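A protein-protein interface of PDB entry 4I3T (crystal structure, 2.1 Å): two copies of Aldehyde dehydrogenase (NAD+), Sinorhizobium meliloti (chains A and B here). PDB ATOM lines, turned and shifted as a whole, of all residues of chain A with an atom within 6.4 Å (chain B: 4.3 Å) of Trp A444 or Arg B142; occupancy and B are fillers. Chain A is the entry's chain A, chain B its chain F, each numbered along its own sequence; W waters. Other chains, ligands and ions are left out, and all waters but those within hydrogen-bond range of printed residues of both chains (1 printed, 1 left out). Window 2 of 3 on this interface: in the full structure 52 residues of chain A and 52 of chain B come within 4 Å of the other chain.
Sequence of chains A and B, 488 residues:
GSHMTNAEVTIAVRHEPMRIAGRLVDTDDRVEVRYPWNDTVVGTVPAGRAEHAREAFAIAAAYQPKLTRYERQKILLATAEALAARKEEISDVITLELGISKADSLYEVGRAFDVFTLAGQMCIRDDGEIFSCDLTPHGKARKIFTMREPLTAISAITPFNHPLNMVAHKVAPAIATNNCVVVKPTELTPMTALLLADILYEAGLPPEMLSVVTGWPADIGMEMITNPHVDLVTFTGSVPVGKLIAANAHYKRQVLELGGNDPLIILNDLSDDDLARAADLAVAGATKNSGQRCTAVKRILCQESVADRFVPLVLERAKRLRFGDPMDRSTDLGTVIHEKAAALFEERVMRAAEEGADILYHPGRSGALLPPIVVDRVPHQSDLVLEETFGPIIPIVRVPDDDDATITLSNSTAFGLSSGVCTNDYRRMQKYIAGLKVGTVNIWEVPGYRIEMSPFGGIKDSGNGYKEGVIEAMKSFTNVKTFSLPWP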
ATOM      1  N   LEU A 264      -3.198  13.816 -12.911  1.00  0.00           N
ATOM      2  CA  LEU A 264      -4.208  14.729 -12.428  1.00  0.00           C
ATOM      3  C   LEU A 264      -5.360  14.554 -13.415  1.00  0.00           C
ATOM      4  O   LEU A 264      -5.208  14.788 -14.616  1.00  0.00           O
ATOM      5  CB  LEU A 264      -3.721  16.171 -12.418  1.00  0.00           C
ATOM      6  CG  LEU A 264      -4.783  17.176 -11.965  1.00  0.00           C
ATOM      7  CD1 LEU A 264      -5.114  16.947 -10.488  1.00  0.00           C
ATOM      8  CD2 LEU A 264      -4.325  18.635 -12.188  1.00  0.00           C
ATOM      9  N   LEU A 270     -17.053  19.682 -14.771  1.00  0.00           N
ATOM     10  CA  LEU A 270     -16.560  20.959 -14.241  1.00  0.00           C
ATOM     11  C   LEU A 270     -17.008  22.168 -15.055  1.00  0.00           C
ATOM     12  O   LEU A 270     -16.998  22.120 -16.274  1.00  0.00           O
ATOM     13  CB  LEU A 270     -15.032  20.949 -14.151  1.00  0.00           C
ATOM     14  CG  LEU A 270     -14.424  19.919 -13.195  1.00  0.00           C
ATOM     15  CD1 LEU A 270     -12.905  20.097 -13.158  1.00  0.00           C
ATOM     16  CD2 LEU A 270     -15.037  20.082 -11.797  1.00  0.00           C
ATOM     17  N   ASP A 273     -15.054  28.001 -14.464  1.00  0.00           N
ATOM     18  CA  ASP A 273     -14.339  28.521 -13.275  1.00  0.00           C
ATOM     19  C   ASP A 273     -13.547  27.377 -12.647  1.00  0.00           C
ATOM     20  O   ASP A 273     -12.380  27.523 -12.271  1.00  0.00           O
ATOM     21  CB  ASP A 273     -15.308  29.095 -12.226  1.00  0.00           C
ATOM     22  CG  ASP A 273     -15.836  30.463 -12.591  1.00  0.00           C
ATOM     23  OD1 ASP A 273     -15.259  31.109 -13.497  1.00  0.00           O
ATOM     24  OD2 ASP A 273     -16.836  30.889 -11.963  1.00  0.00           O
ATOM     25  N   ASP A 274     -14.208  26.231 -12.513  1.00  0.00           N
ATOM     26  CA  ASP A 274     -13.524  25.064 -11.969  1.00  0.00           C
ATOM     27  C   ASP A 274     -12.381  24.606 -12.864  1.00  0.00           C
ATOM     28  O   ASP A 274     -11.336  24.168 -12.366  1.00  0.00           O
ATOM     29  CB  ASP A 274     -14.497  23.918 -11.704  1.00  0.00           C
ATOM     30  CG  ASP A 274     -15.307  24.138 -10.435  1.00  0.00           C
ATOM     31  OD1 ASP A 274     -14.853  24.880  -9.541  1.00  0.00           O
ATOM     32  OD2 ASP A 274     -16.401  23.577 -10.322  1.00  0.00           O
ATOM     33  N   LEU A 275     -12.553  24.714 -14.184  1.00  0.00           N
ATOM     34  CA  LEU A 275     -11.428  24.370 -15.070  1.00  0.00           C
ATOM     35  C   LEU A 275     -10.200  25.241 -14.798  1.00  0.00           C
ATOM     36  O   LEU A 275      -9.055  24.756 -14.827  1.00  0.00           O
ATOM     37  CB  LEU A 275     -11.821  24.425 -16.548  1.00  0.00           C
ATOM     38  CG  LEU A 275     -12.832  23.348 -16.959  1.00  0.00           C
ATOM     39  CD1 LEU A 275     -13.348  23.584 -18.356  1.00  0.00           C
ATOM     40  CD2 LEU A 275     -12.202  21.947 -16.820  1.00  0.00           C
ATOM     41  N   ARG A 277      -9.418  26.574 -11.907  1.00  0.00           N
ATOM     42  CA  ARG A 277      -8.822  26.100 -10.657  1.00  0.00           C
ATOM     43  C   ARG A 277      -8.059  24.806 -10.916  1.00  0.00           C
ATOM     44  O   ARG A 277      -6.960  24.606 -10.400  1.00  0.00           O
ATOM     45  CB  ARG A 277      -9.873  25.884  -9.564  1.00  0.00           C
ATOM     46  CG  ARG A 277     -10.637  27.145  -9.165  1.00  0.00           C
ATOM     47  CD  ARG A 277     -11.173  27.071  -7.735  1.00  0.00           C
ATOM     48  NE  ARG A 277     -12.211  26.050  -7.531  1.00  0.00           N
ATOM     49  CZ  ARG A 277     -12.120  25.021  -6.677  1.00  0.00           C
ATOM     50  NH1 ARG A 277     -11.026  24.850  -5.937  1.00  0.00           N
ATOM     51  NH2 ARG A 277     -13.126  24.156  -6.564  1.00  0.00           N
ATOM     52  N   ALA A 278      -8.641  23.925 -11.733  1.00  0.00           N
ATOM     53  CA  ALA A 278      -7.943  22.697 -12.102  1.00  0.00           C
ATOM     54  C   ALA A 278      -6.650  22.964 -12.884  1.00  0.00           C
ATOM     55  O   ALA A 278      -5.671  22.231 -12.738  1.00  0.00           O
ATOM     56  CB  ALA A 278      -8.857  21.768 -12.891  1.00  0.00           C
ATOM     57  N   ALA A 279      -6.668  23.994 -13.726  1.00  0.00           N
ATOM     58  CA  ALA A 279      -5.489  24.358 -14.480  1.00  0.00           C
ATOM     59  C   ALA A 279      -4.392  24.825 -13.522  1.00  0.00           C
ATOM     60  O   ALA A 279      -3.240  24.535 -13.734  1.00  0.00           O
ATOM     61  CB  ALA A 279      -5.813  25.439 -15.509  1.00  0.00           C
ATOM     62  N   LEU A 281      -3.869  23.817 -10.495  1.00  0.00           N
ATOM     63  CA  LEU A 281      -3.324  22.592  -9.922  1.00  0.00           C
ATOM     64  C   LEU A 281      -2.419  21.888 -10.905  1.00  0.00           C
ATOM     65  O   LEU A 281      -1.359  21.414 -10.541  1.00  0.00           O
ATOM     66  CB  LEU A 281      -4.452  21.633  -9.509  1.00  0.00           C
ATOM     67  CG  LEU A 281      -5.296  22.118  -8.323  1.00  0.00           C
ATOM     68  CD1 LEU A 281      -6.470  21.158  -8.095  1.00  0.00           C
ATOM     69  CD2 LEU A 281      -4.438  22.269  -7.066  1.00  0.00           C
ATOM     70  N   GLY A 420      -4.540  12.790  -8.420  1.00  0.00           N
ATOM     71  CA  GLY A 420      -5.503  13.829  -8.091  1.00  0.00           C
ATOM     72  C   GLY A 420      -6.679  13.745  -9.059  1.00  0.00           C
ATOM     73  O   GLY A 420      -6.483  13.428 -10.227  1.00  0.00           O
ATOM     74  N   VAL A 421      -7.889  14.027  -8.575  1.00  0.00           N
ATOM     75  CA  VAL A 421      -9.084  14.017  -9.411  1.00  0.00           C
ATOM     76  C   VAL A 421      -9.906  15.268  -9.154  1.00  0.00           C
ATOM     77  O   VAL A 421     -10.250  15.555  -8.018  1.00  0.00           O
ATOM     78  CB  VAL A 421      -9.969  12.812  -9.099  1.00  0.00           C
ATOM     79  CG1 VAL A 421     -11.173  12.770 -10.073  1.00  0.00           C
ATOM     80  CG2 VAL A 421      -9.159  11.539  -9.170  1.00  0.00           C
ATOM     81  N   CYS A 422     -10.203  16.020 -10.207  1.00  0.00           N
ATOM     82  CA  CYS A 422     -11.010  17.227 -10.065  1.00  0.00           C
ATOM     83  C   CYS A 422     -12.426  16.972 -10.596  1.00  0.00           C
ATOM     84  O   CYS A 422     -12.603  16.684 -11.784  1.00  0.00           O
ATOM     85  CB  CYS A 422     -10.371  18.406 -10.805  1.00  0.00           C
ATOM     86  SG  CYS A 422      -8.658  18.786 -10.282  1.00  0.00           S
ATOM     87  N   THR A 423     -13.414  17.088  -9.713  1.00  0.00           N
ATOM     88  CA  THR A 423     -14.812  16.837 -10.048  1.00  0.00           C
ATOM     89  C   THR A 423     -15.639  17.261  -8.864  1.00  0.00           C
ATOM     90  O   THR A 423     -15.111  17.349  -7.753  1.00  0.00           O
ATOM     91  CB  THR A 423     -15.078  15.336 -10.293  1.00  0.00           C
ATOM     92  OG1 THR A 423     -16.449  15.151 -10.636  1.00  0.00           O
ATOM     93  CG2 THR A 423     -14.802  14.505  -9.034  1.00  0.00           C
ATOM     94  N   ASN A 424     -16.924  17.526  -9.087  1.00  0.00           N
ATOM     95  CA  ASN A 424     -17.828  17.940  -8.006  1.00  0.00           C
ATOM     96  C   ASN A 424     -18.900  16.897  -7.780  1.00  0.00           C
ATOM     97  O   ASN A 424     -19.747  17.024  -6.914  1.00  0.00           O
ATOM     98  CB  ASN A 424     -18.477  19.282  -8.323  1.00  0.00           C
ATOM     99  CG  ASN A 424     -17.449  20.402  -8.520  1.00  0.00           C
ATOM    100  OD1 ASN A 424     -16.509  20.572  -7.729  1.00  0.00           O
ATOM    101  ND2 ASN A 424     -17.621  21.158  -9.586  1.00  0.00           N
ATOM    102  N   MET A 429     -16.410  10.864  -7.791  1.00  0.00           N
ATOM    103  CA  MET A 429     -15.352  10.917  -6.799  1.00  0.00           C
ATOM    104  C   MET A 429     -15.095   9.528  -6.208  1.00  0.00           C
ATOM    105  O   MET A 429     -13.968   9.025  -6.241  1.00  0.00           O
ATOM    106  CB  MET A 429     -15.767  11.832  -5.663  1.00  0.00           C
ATOM    107  CG  MET A 429     -14.913  12.988  -5.442  1.00  0.00           C
ATOM    108  SD  MET A 429     -15.726  14.028  -4.246  1.00  0.00           S
ATOM    109  CE  MET A 429     -15.967  15.519  -5.215  1.00  0.00           C
ATOM    110  N   ASN A 442      -6.198  12.077  -4.159  1.00  0.00           N
ATOM    111  CA  ASN A 442      -6.565  13.410  -3.662  1.00  0.00           C
ATOM    112  C   ASN A 442      -7.660  14.040  -4.515  1.00  0.00           C
ATOM    113  O   ASN A 442      -7.510  14.192  -5.726  1.00  0.00           O
ATOM    114  CB  ASN A 442      -5.348  14.346  -3.646  1.00  0.00           C
ATOM    115  CG  ASN A 442      -4.352  13.989  -2.555  1.00  0.00           C
ATOM    116  OD1 ASN A 442      -4.736  13.586  -1.444  1.00  0.00           O
ATOM    117  ND2 ASN A 442      -3.064  14.142  -2.865  1.00  0.00           N
ATOM    118  N   ILE A 443      -8.763  14.406  -3.893  1.00  0.00           N
ATOM    119  CA  ILE A 443      -9.851  15.040  -4.636  1.00  0.00           C
ATOM    120  C   ILE A 443      -9.609  16.537  -4.607  1.00  0.00           C
ATOM    121  O   ILE A 443      -9.468  17.138  -3.536  1.00  0.00           O
ATOM    122  CB  ILE A 443     -11.228  14.685  -4.025  1.00  0.00           C
ATOM    123  CG1 ILE A 443     -11.442  13.163  -4.033  1.00  0.00           C
ATOM    124  CG2 ILE A 443     -12.361  15.427  -4.752  1.00  0.00           C
ATOM    125  CD1 ILE A 443     -11.359  12.548  -5.439  1.00  0.00           C
ATOM    126  N   TRP A 444      -9.513  17.133  -5.787  1.00  0.00           N
ATOM    127  CA  TRP A 444      -9.255  18.571  -5.877  1.00  0.00           C
ATOM    128  C   TRP A 444      -7.920  19.024  -5.258  1.00  0.00           C
ATOM    129  O   TRP A 444      -7.820  20.101  -4.666  1.00  0.00           O
ATOM    130  CB  TRP A 444     -10.429  19.369  -5.282  1.00  0.00           C
ATOM    131  CG  TRP A 444     -11.456  19.729  -6.306  1.00  0.00           C
ATOM    132  CD1 TRP A 444     -12.762  19.305  -6.363  1.00  0.00           C
ATOM    133  CD2 TRP A 444     -11.260  20.569  -7.447  1.00  0.00           C
ATOM    134  NE1 TRP A 444     -13.384  19.849  -7.452  1.00  0.00           N
ATOM    135  CE2 TRP A 444     -12.489  20.629  -8.139  1.00  0.00           C
ATOM    136  CE3 TRP A 444     -10.172  21.283  -7.942  1.00  0.00           C
ATOM    137  CZ2 TRP A 444     -12.660  21.383  -9.309  1.00  0.00           C
ATOM    138  CZ3 TRP A 444     -10.335  22.039  -9.094  1.00  0.00           C
ATOM    139  CH2 TRP A 444     -11.580  22.088  -9.764  1.00  0.00           C
ATOM    140  N   GLU A 445      -6.891  18.207  -5.405  1.00  0.00           N
ATOM    141  CA  GLU A 445      -5.531  18.604  -5.048  1.00  0.00           C
ATOM    142  C   GLU A 445      -4.590  17.827  -5.931  1.00  0.00           C
ATOM    143  O   GLU A 445      -4.997  16.851  -6.572  1.00  0.00           O
ATOM    144  CB  GLU A 445      -5.209  18.298  -3.575  1.00  0.00           C
ATOM    145  CG  GLU A 445      -5.123  19.531  -2.684  1.00  0.00           C
ATOM    146  CD  GLU A 445      -4.022  20.536  -3.110  1.00  0.00           C
ATOM    147  OE1 GLU A 445      -3.129  20.170  -3.917  1.00  0.00           O
ATOM    148  OE2 GLU A 445      -4.058  21.699  -2.634  1.00  0.00           O
ATOM    149  N   VAL A 446      -3.325  18.228  -5.964  1.00  0.00           N
ATOM    150  CA  VAL A 446      -2.378  17.543  -6.817  1.00  0.00           C
ATOM    151  C   VAL A 446      -2.020  16.215  -6.167  1.00  0.00           C
ATOM    152  O   VAL A 446      -2.185  16.038  -4.954  1.00  0.00           O
ATOM    153  CB  VAL A 446      -1.095  18.371  -7.026  1.00  0.00           C
ATOM    154  CG1 VAL A 446      -1.404  19.633  -7.830  1.00  0.00           C
ATOM    155  CG2 VAL A 446      -0.451  18.715  -5.673  1.00  0.00           C
ATOM    156  N   TYR A 449      -0.008  16.181  -2.874  1.00  0.00           N
ATOM    157  CA  TYR A 449      -0.473  16.731  -1.618  1.00  0.00           C
ATOM    158  C   TYR A 449      -0.556  15.666  -0.536  1.00  0.00           C
ATOM    159  O   TYR A 449      -1.101  14.595  -0.763  1.00  0.00           O
ATOM    160  CB  TYR A 449      -1.827  17.427  -1.734  1.00  0.00           C
ATOM    161  CG  TYR A 449      -2.244  17.886  -0.374  1.00  0.00           C
ATOM    162  CD1 TYR A 449      -1.718  19.055   0.156  1.00  0.00           C
ATOM    163  CD2 TYR A 449      -3.082  17.110   0.423  1.00  0.00           C
ATOM    164  CE1 TYR A 449      -2.045  19.475   1.427  1.00  0.00           C
ATOM    165  CE2 TYR A 449      -3.422  17.524   1.706  1.00  0.00           C
ATOM    166  CZ  TYR A 449      -2.896  18.709   2.201  1.00  0.00           C
ATOM    167  OH  TYR A 449      -3.205  19.143   3.466  1.00  0.00           O
ATOM    168  N   PHE B 131      -7.333  12.156   9.392  1.00  0.00           N
ATOM    169  CA  PHE B 131      -6.387  13.203   9.753  1.00  0.00           C
ATOM    170  C   PHE B 131      -6.940  14.544   9.343  1.00  0.00           C
ATOM    171  O   PHE B 131      -7.442  14.695   8.227  1.00  0.00           O
ATOM    172  CB  PHE B 131      -5.060  13.026   9.024  1.00  0.00           C
ATOM    173  CG  PHE B 131      -4.358  11.757   9.332  1.00  0.00           C
ATOM    174  CD1 PHE B 131      -3.360  11.720  10.300  1.00  0.00           C
ATOM    175  CD2 PHE B 131      -4.672  10.588   8.642  1.00  0.00           C
ATOM    176  CE1 PHE B 131      -2.688  10.544  10.584  1.00  0.00           C
ATOM    177  CE2 PHE B 131      -3.995   9.383   8.923  1.00  0.00           C
ATOM    178  CZ  PHE B 131      -3.005   9.368   9.901  1.00  0.00           C
ATOM    179  N   SER B 132      -6.846  15.524  10.239  1.00  0.00           N
ATOM    180  CA  SER B 132      -7.137  16.904   9.879  1.00  0.00           C
ATOM    181  C   SER B 132      -5.867  17.546   9.318  1.00  0.00           C
ATOM    182  O   SER B 132      -4.749  17.234   9.747  1.00  0.00           O
ATOM    183  CB  SER B 132      -7.685  17.684  11.078  1.00  0.00           C
ATOM    184  OG  SER B 132      -9.033  17.328  11.320  1.00  0.00           O
ATOM    185  N   CYS B 133      -6.018  18.443   8.358  1.00  0.00           N
ATOM    186  CA  CYS B 133      -4.858  18.920   7.616  1.00  0.00           C
ATOM    187  C   CYS B 133      -4.397  20.356   7.908  1.00  0.00           C
ATOM    188  O   CYS B 133      -3.412  20.796   7.328  1.00  0.00           O
ATOM    189  CB  CYS B 133      -5.106  18.770   6.109  1.00  0.00           C
ATOM    190  SG  CYS B 133      -5.201  17.026   5.527  1.00  0.00           S
ATOM    191  N   LYS B 140      -4.104  22.893   5.133  1.00  0.00           N
ATOM    192  CA  LYS B 140      -5.270  23.129   4.286  1.00  0.00           C
ATOM    193  C   LYS B 140      -6.528  22.721   5.031  1.00  0.00           C
ATOM    194  O   LYS B 140      -6.479  21.852   5.912  1.00  0.00           O
ATOM    195  CB  LYS B 140      -5.156  22.284   3.013  1.00  0.00           C
ATOM    196  CG  LYS B 140      -3.975  22.646   2.122  1.00  0.00           C
ATOM    197  CD  LYS B 140      -4.290  23.897   1.298  1.00  0.00           C
ATOM    198  CE  LYS B 140      -3.074  24.404   0.523  1.00  0.00           C
ATOM    199  NZ  LYS B 140      -2.434  23.313  -0.284  1.00  0.00           N
ATOM    200  N   ALA B 141      -7.655  23.335   4.677  1.00  0.00           N
ATOM    201  CA  ALA B 141      -8.928  22.942   5.267  1.00  0.00           C
ATOM    202  C   ALA B 141      -9.393  21.680   4.537  1.00  0.00           C
ATOM    203  O   ALA B 141     -10.131  21.743   3.556  1.00  0.00           O
ATOM    204  CB  ALA B 141      -9.942  24.047   5.135  1.00  0.00           C
ATOM    205  N   ARG B 142      -8.962  20.534   5.042  1.00  0.00           N
ATOM    206  CA  ARG B 142      -9.024  19.289   4.307  1.00  0.00           C
ATOM    207  C   ARG B 142      -8.890  18.107   5.277  1.00  0.00           C
ATOM    208  O   ARG B 142      -8.297  18.242   6.357  1.00  0.00           O
ATOM    209  CB  ARG B 142      -7.891  19.296   3.275  1.00  0.00           C
ATOM    210  CG  ARG B 142      -7.624  17.976   2.566  1.00  0.00           C
ATOM    211  CD  ARG B 142      -6.667  18.178   1.349  1.00  0.00           C
ATOM    212  NE  ARG B 142      -7.297  19.030   0.337  1.00  0.00           N
ATOM    213  CZ  ARG B 142      -7.961  18.573  -0.724  1.00  0.00           C
ATOM    214  NH1 ARG B 142      -8.030  17.264  -0.946  1.00  0.00           N
ATOM    215  NH2 ARG B 142      -8.523  19.419  -1.590  1.00  0.00           N
ATOM    216  N   LYS B 143      -9.458  16.956   4.908  1.00  0.00           N
ATOM    217  CA  LYS B 143      -9.335  15.762   5.734  1.00  0.00           C
ATOM    218  C   LYS B 143      -8.740  14.648   4.884  1.00  0.00           C
ATOM    219  O   LYS B 143      -9.042  14.517   3.688  1.00  0.00           O
ATOM    220  CB  LYS B 143     -10.681  15.326   6.346  1.00  0.00           C
ATOM    221  CG  LYS B 143     -11.213  16.228   7.477  1.00  0.00           C
ATOM    222  CD  LYS B 143     -12.554  15.705   8.005  1.00  0.00           C
ATOM    223  CE  LYS B 143     -13.071  16.518   9.216  1.00  0.00           C
ATOM    224  NZ  LYS B 143     -12.303  16.213  10.467  1.00  0.00           N
ATOM    225  N   SER B 484      -8.142  12.194   0.257  1.00  0.00           N
ATOM    226  CA  SER B 484      -8.409  13.446   0.952  1.00  0.00           C
ATOM    227  C   SER B 484      -9.541  14.176   0.255  1.00  0.00           C
ATOM    228  O   SER B 484      -9.671  14.092  -0.968  1.00  0.00           O
ATOM    229  CB  SER B 484      -7.142  14.331   1.035  1.00  0.00           C
ATOM    230  OG  SER B 484      -6.723  14.743  -0.263  1.00  0.00           O
ATOM    231  N   LEU B 485     -10.361  14.849   1.055  1.00  0.00           N
ATOM    232  CA  LEU B 485     -11.455  15.672   0.583  1.00  0.00           C
ATOM    233  C   LEU B 485     -11.307  17.109   1.089  1.00  0.00           C
ATOM    234  O   LEU B 485     -10.884  17.323   2.218  1.00  0.00           O
ATOM    235  CB  LEU B 485     -12.774  15.107   1.110  1.00  0.00           C
ATOM    236  CG  LEU B 485     -13.066  13.642   0.755  1.00  0.00           C
ATOM    237  CD1 LEU B 485     -14.336  13.137   1.426  1.00  0.00           C
ATOM    238  CD2 LEU B 485     -13.182  13.505  -0.748  1.00  0.00           C
ATOM    239  N   PRO B 486     -11.696  18.093   0.261  1.00  0.00           N
ATOM    240  CA  PRO B 486     -11.838  19.464   0.764  1.00  0.00           C
ATOM    241  C   PRO B 486     -12.754  19.455   1.968  1.00  0.00           C
ATOM    242  O   PRO B 486     -13.790  18.794   1.940  1.00  0.00           O
ATOM    243  CB  PRO B 486     -12.507  20.221  -0.403  1.00  0.00           C
ATOM    244  CG  PRO B 486     -12.177  19.392  -1.642  1.00  0.00           C
ATOM    245  CD  PRO B 486     -12.135  17.950  -1.143  1.00  0.00           C
ATOM    246  N   TRP B 487     -12.377  20.175   3.015  1.00  0.00           N
ATOM    247  CA  TRP B 487     -13.241  20.283   4.172  1.00  0.00           C
ATOM    248  C   TRP B 487     -13.309  21.734   4.686  1.00  0.00           C
ATOM    249  O   TRP B 487     -12.801  22.028   5.762  1.00  0.00           O
ATOM    250  CB  TRP B 487     -12.786  19.314   5.272  1.00  0.00           C
ATOM    251  CG  TRP B 487     -13.912  18.923   6.156  1.00  0.00           C
ATOM    252  CD1 TRP B 487     -14.300  19.525   7.320  1.00  0.00           C
ATOM    253  CD2 TRP B 487     -14.834  17.859   5.923  1.00  0.00           C
ATOM    254  NE1 TRP B 487     -15.415  18.893   7.827  1.00  0.00           N
ATOM    255  CE2 TRP B 487     -15.758  17.865   6.991  1.00  0.00           C
ATOM    256  CE3 TRP B 487     -14.971  16.903   4.913  1.00  0.00           C
ATOM    257  CZ2 TRP B 487     -16.799  16.939   7.085  1.00  0.00           C
ATOM    258  CZ3 TRP B 487     -16.013  15.982   5.005  1.00  0.00           C
ATOM    259  CH2 TRP B 487     -16.915  16.014   6.086  1.00  0.00           C
HETATM  260  O   HOH W   1      -2.417  21.122   4.587  1.00  0.00           O
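OD1 of Asn A442 lies within hydrogen-bond range of OG of Ser B484 (2.6 Å). O of Ile A443 sits at hydrogen-bond distance from NH1 of Arg B142. N of Ile A443 sits at hydrogen-bond distance from O of Ser B484, at 3.1 Å. The backbone carbonyl oxygen (O) of Trp A444 lies within hydrogen-bond range of the guanidinium group (NH2) of Arg B142, 3.2 Å away. The side-chain amino group of Lys B140 lies within salt-bridge range of the side-chain carboxylate of Glu A445, 3.3 Å away. SG of Cys B133 lies close to OH of Tyr A449, at 3.6 Å.
The backbone carbonyl oxygen (O) of Asn A442 sits at hydrogen-bond distance from the backbone NH (N) of Val A421 (2.9 Å). O of Val A446 sits at hydrogen-bond distance from ND2 of Asn A442 (3.0 Å). O of Cys B133 sits at hydrogen-bond distance from N of Lys B140, at 3.1 Å. The backbone NH of Cys B133 is in hydrogen-bond range of the backbone carbonyl oxygen of Arg B142 (3.0 Å). The guanidinium group (NH1) of Arg B142 sits at hydrogen-bond distance from the side-chain hydroxyl (OG) of Ser B484 (2.9 Å). O of Lys B143 is in hydrogen-bond range of N of Leu B485.
Among the printed residues, pairs that only touch across the chains: Tyr A449 with Arg B142 (3.3 Å), Glu A445 with Arg B142 (3.6 Å), Ile A443 with Pro B486 (3.7 Å), Tyr A449 with Lys B140 (3.7 Å) and Ile A443 with Leu B485 (3.7 Å).
Printed residues of chain B within 4 Å of Asn A442: Ser B484. Of the printed residues of chain B, Ile A443 touches Arg B142 (3.0 Å), Ser B484 (3.1 Å), Leu B485 (3.7 Å) and Pro B486 (3.7 Å). Of chain B, only Arg B142 comes within 4 Å of Trp A444. Of the printed residues of chain B, Glu A445 touches Lys B140 and Arg B142. Printed residues of chain A within 4 Å of Cys B133: Tyr A449. Arg B142 touches just these residues of chain A: Ile A443 (3.0 Å), Trp A444 (3.2 Å), Glu A445 (3.6 Å) and Tyr A449 (3.3 Å). Of the printed residues of chain A, Pro B486 touches Ile A443. The nearest residue of chain B that does not touch Trp A444 is Pro B486 (4.04 Å). The nearest printed residue of chain A that does not touch Cys B133 is Asn A442 (7.8 Å).
Printed residues of chain A that touch a printed residue of chain B: Asn A442, Ile A443, Trp A444, Glu A445 and Tyr A449. Among the printed residues, 11 pairs touch across the chains. Among the printed residues, Asp or Glu carboxylates within 4 Å of a Lys or Arg side-chain nitrogen of the other chain: Glu A445 with Lys B140 (3.3 Å).
No position is printed for both chains. Of the 11 pairs that touch across the chains among the printed residues, none has its exchanged pair printed and touching as well.
Water W1 lies within hydrogen-bond range of OH of Tyr A449, N of Lys B140 and O of Cys B133.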
